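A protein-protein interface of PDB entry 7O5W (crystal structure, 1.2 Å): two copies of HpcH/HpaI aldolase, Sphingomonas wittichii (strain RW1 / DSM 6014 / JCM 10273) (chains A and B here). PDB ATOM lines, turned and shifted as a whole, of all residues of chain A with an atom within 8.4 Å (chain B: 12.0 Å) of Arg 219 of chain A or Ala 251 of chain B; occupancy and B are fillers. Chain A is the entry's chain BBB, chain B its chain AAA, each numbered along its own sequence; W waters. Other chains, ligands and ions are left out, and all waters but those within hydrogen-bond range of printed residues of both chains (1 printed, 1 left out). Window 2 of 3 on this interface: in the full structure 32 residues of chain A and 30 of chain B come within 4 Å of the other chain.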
ATOM      1  N   LEU A  16     -24.282 -15.477   9.516  1.00  0.00           N
ATOM      2  CA  LEU A  16     -23.141 -14.577   9.695  1.00  0.00           C
ATOM      3  C   LEU A  16     -23.703 -13.218  10.122  1.00  0.00           C
ATOM      4  O   LEU A  16     -24.634 -12.706   9.484  1.00  0.00           O
ATOM      5  CB  LEU A  16     -22.345 -14.399   8.399  1.00  0.00           C
ATOM      6  CG  LEU A  16     -21.130 -13.490   8.479  1.00  0.00           C
ATOM      7  CD1 LEU A  16     -20.024 -14.122   9.314  1.00  0.00           C
ATOM      8  CD2 LEU A  16     -20.625 -13.159   7.108  1.00  0.00           C
ATOM      9  N   CYS A 212     -15.972 -13.302  16.495  1.00  0.00           N
ATOM     10  CA  CYS A 212     -14.719 -13.253  15.764  1.00  0.00           C
ATOM     11  C   CYS A 212     -14.300 -11.830  15.483  1.00  0.00           C
ATOM     12  O   CYS A 212     -15.099 -10.924  15.300  1.00  0.00           O
ATOM     13  CB  CYS A 212     -14.840 -13.975  14.430  1.00  0.00           C
ATOM     14  SG  CYS A 212     -15.458 -15.653  14.522  1.00  0.00           S
ATOM     15  N   SER A 214     -12.168 -11.067  12.883  1.00  0.00           N
ATOM     16  CA  SER A 214     -11.632 -11.050  11.520  1.00  0.00           C
ATOM     17  C   SER A 214     -12.451 -11.959  10.629  1.00  0.00           C
ATOM     18  O   SER A 214     -13.066 -12.934  11.107  1.00  0.00           O
ATOM     19  CB  SER A 214     -10.201 -11.480  11.484  1.00  0.00           C
ATOM     20  OG  SER A 214     -10.049 -12.825  11.896  1.00  0.00           O
ATOM     21  N   GLY A 215     -12.456 -11.642   9.361  1.00  0.00           N
ATOM     22  CA  GLY A 215     -13.076 -12.516   8.364  1.00  0.00           C
ATOM     23  C   GLY A 215     -12.411 -13.869   8.293  1.00  0.00           C
ATOM     24  O   GLY A 215     -13.065 -14.885   8.099  1.00  0.00           O
ATOM     25  N   GLY A 216     -11.092 -13.914   8.392  1.00  0.00           N
ATOM     26  CA  GLY A 216     -10.350 -15.167   8.305  1.00  0.00           C
ATOM     27  C   GLY A 216     -10.734 -16.134   9.441  1.00  0.00           C
ATOM     28  O   GLY A 216     -10.892 -17.329   9.225  1.00  0.00           O
ATOM     29  N   PHE A 217     -10.780 -15.626  10.669  1.00  0.00           N
ATOM     30  CA  PHE A 217     -11.170 -16.469  11.815  1.00  0.00           C
ATOM     31  C   PHE A 217     -12.620 -16.895  11.664  1.00  0.00           C
ATOM     32  O   PHE A 217     -12.930 -18.095  11.927  1.00  0.00           O
ATOM     33  CB  PHE A 217     -10.856 -15.756  13.144  1.00  0.00           C
ATOM     34  CG  PHE A 217     -10.996 -16.591  14.388  1.00  0.00           C
ATOM     35  CD1 PHE A 217      -9.951 -17.316  14.911  1.00  0.00           C
ATOM     36  CD2 PHE A 217     -12.182 -16.606  15.128  1.00  0.00           C
ATOM     37  CE1 PHE A 217     -10.103 -18.085  16.059  1.00  0.00           C
ATOM     38  CE2 PHE A 217     -12.327 -17.315  16.292  1.00  0.00           C
ATOM     39  CZ  PHE A 217     -11.277 -18.026  16.764  1.00  0.00           C
ATOM     40  N   ALA A 218     -13.476 -15.990  11.214  1.00  0.00           N
ATOM     41  CA  ALA A 218     -14.884 -16.370  10.988  1.00  0.00           C
ATOM     42  C   ALA A 218     -14.994 -17.471   9.957  1.00  0.00           C
ATOM     43  O   ALA A 218     -15.844 -18.382  10.082  1.00  0.00           O
ATOM     44  CB  ALA A 218     -15.643 -15.171  10.502  1.00  0.00           C
ATOM     45  N   ARG A 219     -14.202 -17.433   8.914  1.00  0.00           N
ATOM     46  CA  ARG A 219     -14.267 -18.477   7.892  1.00  0.00           C
ATOM     47  C   ARG A 219     -13.939 -19.842   8.540  1.00  0.00           C
ATOM     48  O   ARG A 219     -14.582 -20.844   8.227  1.00  0.00           O
ATOM     49  CB  ARG A 219     -13.241 -18.125   6.826  1.00  0.00           C
ATOM     50  CG  ARG A 219     -13.097 -19.139   5.743  1.00  0.00           C
ATOM     51  CD  ARG A 219     -12.061 -18.612   4.776  1.00  0.00           C
ATOM     52  NE  ARG A 219     -11.887 -19.514   3.670  1.00  0.00           N
ATOM     53  CZ  ARG A 219     -11.659 -19.083   2.414  1.00  0.00           C
ATOM     54  NH1 ARG A 219     -11.675 -17.786   2.113  1.00  0.00           N
ATOM     55  NH2 ARG A 219     -11.508 -19.969   1.457  1.00  0.00           N
ATOM     56  N   VAL A 220     -12.915 -19.884   9.362  1.00  0.00           N
ATOM     57  CA  VAL A 220     -12.560 -21.132  10.038  1.00  0.00           C
ATOM     58  C   VAL A 220     -13.729 -21.593  10.903  1.00  0.00           C
ATOM     59  O   VAL A 220     -14.051 -22.777  10.960  1.00  0.00           O
ATOM     60  CB  VAL A 220     -11.265 -21.030  10.848  1.00  0.00           C
ATOM     61  CG1 VAL A 220     -10.927 -22.311  11.590  1.00  0.00           C
ATOM     62  CG2 VAL A 220     -10.130 -20.638   9.917  1.00  0.00           C
ATOM     63  N   LYS A 221     -14.321 -20.681  11.667  1.00  0.00           N
ATOM     64  CA  LYS A 221     -15.418 -21.095  12.594  1.00  0.00           C
ATOM     65  C   LYS A 221     -16.606 -21.605  11.802  1.00  0.00           C
ATOM     66  O   LYS A 221     -17.249 -22.599  12.199  1.00  0.00           O
ATOM     67  CB  LYS A 221     -15.780 -19.932  13.496  1.00  0.00           C
ATOM     68  CG  LYS A 221     -14.690 -19.421  14.439  1.00  0.00           C
ATOM     69  CD  LYS A 221     -14.007 -20.438  15.273  1.00  0.00           C
ATOM     70  CE  LYS A 221     -12.700 -20.894  14.675  1.00  0.00           C
ATOM     71  NZ  LYS A 221     -12.008 -21.886  15.548  1.00  0.00           N
ATOM     72  N   LEU A 222     -16.934 -20.948  10.695  1.00  0.00           N
ATOM     73  CA  LEU A 222     -17.996 -21.468   9.826  1.00  0.00           C
ATOM     74  C   LEU A 222     -17.625 -22.902   9.382  1.00  0.00           C
ATOM     75  O   LEU A 222     -18.460 -23.786   9.371  1.00  0.00           O
ATOM     76  CB  LEU A 222     -18.306 -20.518   8.671  1.00  0.00           C
ATOM     77  CG  LEU A 222     -18.929 -19.185   9.096  1.00  0.00           C
ATOM     78  CD1 LEU A 222     -18.772 -18.165   8.013  1.00  0.00           C
ATOM     79  CD2 LEU A 222     -20.389 -19.423   9.410  1.00  0.00           C
ATOM     80  N   ALA A 223     -16.386 -23.110   8.933  1.00  0.00           N
ATOM     81  CA  ALA A 223     -15.916 -24.469   8.508  1.00  0.00           C
ATOM     82  C   ALA A 223     -16.000 -25.482   9.632  1.00  0.00           C
ATOM     83  O   ALA A 223     -16.068 -26.682   9.336  1.00  0.00           O
ATOM     84  CB  ALA A 223     -14.473 -24.382   7.978  1.00  0.00           C
ATOM     85  N   GLU A 224     -15.800 -25.059  10.877  1.00  0.00           N
ATOM     86  CA  GLU A 224     -15.880 -25.952  12.051  1.00  0.00           C
ATOM     87  C   GLU A 224     -17.333 -26.284  12.397  1.00  0.00           C
ATOM     88  O   GLU A 224     -17.484 -27.047  13.395  1.00  0.00           O
ATOM     89  CB  GLU A 224     -15.107 -25.352  13.237  1.00  0.00           C
ATOM     90  CG  GLU A 224     -13.632 -25.384  13.053  1.00  0.00           C
ATOM     91  CD  GLU A 224     -12.795 -24.903  14.222  1.00  0.00           C
ATOM     92  OE1 GLU A 224     -13.399 -24.125  15.019  1.00  0.00           O
ATOM     93  OE2 GLU A 224     -11.566 -25.269  14.343  1.00  0.00           O
ATOM     94  N   GLY A 225     -18.329 -25.696  11.718  1.00  0.00           N
ATOM     95  CA  GLY A 225     -19.746 -25.999  11.948  1.00  0.00           C
ATOM     96  C   GLY A 225     -20.425 -25.122  12.982  1.00  0.00           C
ATOM     97  O   GLY A 225     -21.555 -25.461  13.420  1.00  0.00           O
ATOM     98  N   PHE A 226     -19.879 -23.984  13.326  1.00  0.00           N
ATOM     99  CA  PHE A 226     -20.634 -23.044  14.167  1.00  0.00           C
ATOM    100  C   PHE A 226     -21.881 -22.573  13.446  1.00  0.00           C
ATOM    101  O   PHE A 226     -21.898 -22.341  12.223  1.00  0.00           O
ATOM    102  CB  PHE A 226     -19.721 -21.883  14.631  1.00  0.00           C
ATOM    103  CG  PHE A 226     -18.755 -22.260  15.698  1.00  0.00           C
ATOM    104  CD1 PHE A 226     -17.551 -22.856  15.395  1.00  0.00           C
ATOM    105  CD2 PHE A 226     -19.085 -22.064  17.019  1.00  0.00           C
ATOM    106  CE1 PHE A 226     -16.692 -23.266  16.387  1.00  0.00           C
ATOM    107  CE2 PHE A 226     -18.193 -22.468  17.999  1.00  0.00           C
ATOM    108  CZ  PHE A 226     -17.024 -23.060  17.677  1.00  0.00           C
ATOM    109  N   VAL A 229     -21.999 -16.853  13.600  1.00  0.00           N
ATOM    110  CA  VAL A 229     -20.623 -16.365  13.654  1.00  0.00           C
ATOM    111  C   VAL A 229     -20.684 -14.873  13.446  1.00  0.00           C
ATOM    112  O   VAL A 229     -21.334 -14.426  12.500  1.00  0.00           O
ATOM    113  CB  VAL A 229     -19.772 -17.064  12.573  1.00  0.00           C
ATOM    114  CG1 VAL A 229     -18.391 -16.500  12.456  1.00  0.00           C
ATOM    115  CG2 VAL A 229     -19.679 -18.543  12.819  1.00  0.00           C
ATOM    116  N   THR A 230     -20.019 -14.097  14.315  1.00  0.00           N
ATOM    117  CA  THR A 230     -20.000 -12.654  14.137  1.00  0.00           C
ATOM    118  C   THR A 230     -18.628 -12.203  13.693  1.00  0.00           C
ATOM    119  O   THR A 230     -17.598 -12.714  14.161  1.00  0.00           O
ATOM    120  CB  THR A 230     -20.391 -11.914  15.413  1.00  0.00           C
ATOM    121  OG1 THR A 230     -19.422 -12.043  16.451  1.00  0.00           O
ATOM    122  CG2 THR A 230     -21.696 -12.449  15.949  1.00  0.00           C
ATOM    123  N   ALA A 231     -18.600 -11.244  12.771  1.00  0.00           N
ATOM    124  CA  ALA A 231     -17.310 -10.696  12.311  1.00  0.00           C
ATOM    125  C   ALA A 231     -17.584  -9.398  11.561  1.00  0.00           C
ATOM    126  O   ALA A 231     -18.462  -9.413  10.678  1.00  0.00           O
ATOM    127  CB  ALA A 231     -16.584 -11.625  11.377  1.00  0.00           C
ATOM    128  N   ALA B 242     -16.218  -3.983   5.835  1.00  0.00           N
ATOM    129  CA  ALA B 242     -17.229  -5.009   6.142  1.00  0.00           C
ATOM    130  C   ALA B 242     -17.459  -5.894   4.932  1.00  0.00           C
ATOM    131  O   ALA B 242     -17.584  -7.102   5.117  1.00  0.00           O
ATOM    132  CB  ALA B 242     -18.499  -4.354   6.622  1.00  0.00           C
ATOM    133  N   ARG B 243     -17.540  -5.297   3.757  1.00  0.00           N
ATOM    134  CA  ARG B 243     -17.725  -6.145   2.563  1.00  0.00           C
ATOM    135  C   ARG B 243     -16.602  -7.154   2.462  1.00  0.00           C
ATOM    136  O   ARG B 243     -16.856  -8.321   2.048  1.00  0.00           O
ATOM    137  CB  ARG B 243     -17.824  -5.302   1.312  1.00  0.00           C
ATOM    138  CG  ARG B 243     -19.132  -4.549   1.190  1.00  0.00           C
ATOM    139  CD  ARG B 243     -19.396  -3.911  -0.136  1.00  0.00           C
ATOM    140  NE  ARG B 243     -18.427  -2.934  -0.485  1.00  0.00           N
ATOM    141  CZ  ARG B 243     -18.489  -1.636  -0.162  1.00  0.00           C
ATOM    142  NH1 ARG B 243     -19.464  -1.174   0.573  1.00  0.00           N
ATOM    143  NH2 ARG B 243     -17.503  -0.827  -0.475  1.00  0.00           N
ATOM    144  N   GLN B 244     -15.392  -6.732   2.697  1.00  0.00           N
ATOM    145  CA  GLN B 244     -14.241  -7.651   2.607  1.00  0.00           C
ATOM    146  C   GLN B 244     -14.290  -8.725   3.686  1.00  0.00           C
ATOM    147  O   GLN B 244     -13.987  -9.888   3.414  1.00  0.00           O
ATOM    148  CB  GLN B 244     -12.954  -6.859   2.657  1.00  0.00           C
ATOM    149  CG  GLN B 244     -11.744  -7.742   2.417  1.00  0.00           C
ATOM    150  CD  GLN B 244     -11.767  -8.360   1.038  1.00  0.00           C
ATOM    151  OE1 GLN B 244     -11.807  -7.647   0.038  1.00  0.00           O
ATOM    152  NE2 GLN B 244     -11.731  -9.684   0.979  1.00  0.00           N
ATOM    153  N   VAL B 245     -14.636  -8.339   4.910  1.00  0.00           N
ATOM    154  CA  VAL B 245     -14.763  -9.336   6.006  1.00  0.00           C
ATOM    155  C   VAL B 245     -15.801 -10.387   5.589  1.00  0.00           C
ATOM    156  O   VAL B 245     -15.573 -11.597   5.803  1.00  0.00           O
ATOM    157  CB  VAL B 245     -15.095  -8.663   7.331  1.00  0.00           C
ATOM    158  CG1 VAL B 245     -15.666  -9.654   8.343  1.00  0.00           C
ATOM    159  CG2 VAL B 245     -13.866  -7.949   7.849  1.00  0.00           C
ATOM    160  N   ILE B 246     -16.938  -9.972   5.058  1.00  0.00           N
ATOM    161  CA  ILE B 246     -17.991 -10.910   4.678  1.00  0.00           C
ATOM    162  C   ILE B 246     -17.483 -11.822   3.572  1.00  0.00           C
ATOM    163  O   ILE B 246     -17.718 -13.037   3.608  1.00  0.00           O
ATOM    164  CB  ILE B 246     -19.256 -10.145   4.283  1.00  0.00           C
ATOM    165  CG1 ILE B 246     -19.862  -9.467   5.497  1.00  0.00           C
ATOM    166  CG2 ILE B 246     -20.246 -11.078   3.601  1.00  0.00           C
ATOM    167  CD1 ILE B 246     -20.911  -8.432   5.089  1.00  0.00           C
ATOM    168  N   ALA B 247     -16.818 -11.263   2.568  1.00  0.00           N
ATOM    169  CA  ALA B 247     -16.323 -12.094   1.449  1.00  0.00           C
ATOM    170  C   ALA B 247     -15.336 -13.095   2.008  1.00  0.00           C
ATOM    171  O   ALA B 247     -15.308 -14.271   1.547  1.00  0.00           O
ATOM    172  CB  ALA B 247     -15.675 -11.186   0.425  1.00  0.00           C
ATOM    173  N   ASP B 248     -14.482 -12.691   2.899  1.00  0.00           N
ATOM    174  CA  ASP B 248     -13.477 -13.608   3.471  1.00  0.00           C
ATOM    175  C   ASP B 248     -14.191 -14.705   4.267  1.00  0.00           C
ATOM    176  O   ASP B 248     -13.865 -15.916   4.177  1.00  0.00           O
ATOM    177  CB  ASP B 248     -12.465 -12.863   4.335  1.00  0.00           C
ATOM    178  CG  ASP B 248     -11.526 -11.943   3.519  1.00  0.00           C
ATOM    179  OD1 ASP B 248     -11.461 -12.095   2.290  1.00  0.00           O
ATOM    180  OD2 ASP B 248     -10.870 -11.073   4.131  1.00  0.00           O
ATOM    181  N   ALA B 249     -15.160 -14.342   5.094  1.00  0.00           N
ATOM    182  CA  ALA B 249     -15.869 -15.289   5.968  1.00  0.00           C
ATOM    183  C   ALA B 249     -16.648 -16.305   5.135  1.00  0.00           C
ATOM    184  O   ALA B 249     -16.640 -17.468   5.463  1.00  0.00           O
ATOM    185  CB  ALA B 249     -16.779 -14.500   6.880  1.00  0.00           C
ATOM    186  N   ARG B 250     -17.330 -15.843   4.111  1.00  0.00           N
ATOM    187  CA  ARG B 250     -18.225 -16.687   3.314  1.00  0.00           C
ATOM    188  C   ARG B 250     -17.436 -17.477   2.244  1.00  0.00           C
ATOM    189  O   ARG B 250     -18.037 -18.262   1.580  1.00  0.00           O
ATOM    190  CB  ARG B 250     -19.354 -15.901   2.682  1.00  0.00           C
ATOM    191  CG  ARG B 250     -20.286 -15.301   3.742  1.00  0.00           C
ATOM    192  CD  ARG B 250     -21.580 -14.828   3.128  1.00  0.00           C
ATOM    193  NE  ARG B 250     -22.552 -14.231   4.034  1.00  0.00           N
ATOM    194  CZ  ARG B 250     -23.427 -14.930   4.763  1.00  0.00           C
ATOM    195  NH1 ARG B 250     -23.395 -16.237   4.814  1.00  0.00           N
ATOM    196  NH2 ARG B 250     -24.393 -14.300   5.401  1.00  0.00           N
ATOM    197  N   ALA B 251     -16.151 -17.236   2.092  1.00  0.00           N
ATOM    198  CA  ALA B 251     -15.285 -17.946   1.102  1.00  0.00           C
ATOM    199  C   ALA B 251     -15.841 -17.689  -0.289  1.00  0.00           C
ATOM    200  O   ALA B 251     -15.882 -16.462  -0.420  1.00  0.00           O
ATOM    201  CB  ALA B 251     -15.206 -19.430   1.406  1.00  0.00           C
HETATM  202  O   HOH W   1     -10.898 -15.898   3.719  1.00  0.00           O
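The side-chain carboxylate of Asp 248 of chain B sits at hydrogen-bond distance from the side-chain amide nitrogen of Gln 244 of chain B (2.8 Å).
Leu 16 of chain A touches Arg 250 of chain B (CB to NH2, 3.6 Å). Gly 215 of chain A touches Val 245 of chain B (CA to O, 3.7 Å). Asp 248 of chain B touches Gly 215 of chain A (C to O, 3.998 Å). Ala 249 of chain B touches Gly 215 of chain A (CA to O, 3.5 Å). Ala 249 of chain B touches Ala 218 of chain A. Asp 248 of chain B touches Arg 219 of chain A (O to CD, 3.3 Å). Arg 219 of chain A touches Ala 249 of chain B. CZ of Arg 219 of chain A touches CB of Ala 251 of chain B, at 3.7 Å. CD1 of Leu 222 of chain A touches O of Ala 249 of chain B, 3.4 Å away. CG1 of Val 245 of chain B touches O of Ala 231 of chain A, at 3.7 Å.
Arg 219 of chain A touches just these residues of chain B: Asp 248 (3.3 Å), Ala 249 (3.5 Å) and Ala 251 (3.7 Å). Of chain A, only Arg 219 (3.7 Å) comes within 4 Å of Ala 251 of chain B. No residue of chain B comes within 4 Å of Ser 214 of chain A. No residue of chain B comes within 4 Å of Gly 216 of chain A. Ala 218 of chain A touches just one residue of chain B: Ala 249 (3.9 Å). No residue of chain B comes within 4 Å of Lys 221 of chain A. Leu 222 of chain A touches one residue of chain B. No residue of chain B comes within 4 Å of Ala 223 of chain A. Of the printed residues of chain B, Leu 16 of chain A touches Arg 250 (3.6 Å). Printed residues of chain A within 4 Å of Arg 250 of chain B: Leu 16 (3.6 Å). Of the printed residues of chain B, Gly 215 of chain A touches Val 245, Asp 248 and Ala 249. Printed residues of chain A within 4 Å of Val 245 of chain B: Gly 215 (3.7 Å) and Ala 231 (3.7 Å). Printed residues of chain B within 4 Å of Ala 231 of chain A: Val 245 (3.7 Å). The nearest printed residue of chain A that does not touch Ala 249 of chain B is Leu 16 of chain A (4.1 Å).
Of the 10 printed residues of chain B, 5 touch a printed residue of chain A. Hydrophobic or aromatic side chains of chain B that line the printed part of chain A: Val 245, Ala 249 and Ala 251. Along chain B the printed residues that touch a printed residue of chain A span positions 245 to 251. Hydrophobic or aromatic side chains of chain A within 4 Å of the printed part of chain B: Leu 16, Ala 218, Leu 222 and Ala 231. Among the printed residues, 10 pairs touch across the chains.
No position is printed for both chains. Of the 10 pairs that touch across the chains among the printed residues, none has its exchanged pair printed and touching as well.
Water W1 lies within hydrogen-bond range of NH1 of Arg 219 of chain A (2.6 Å) and O of Asp 248 of chain B (3.0 Å).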
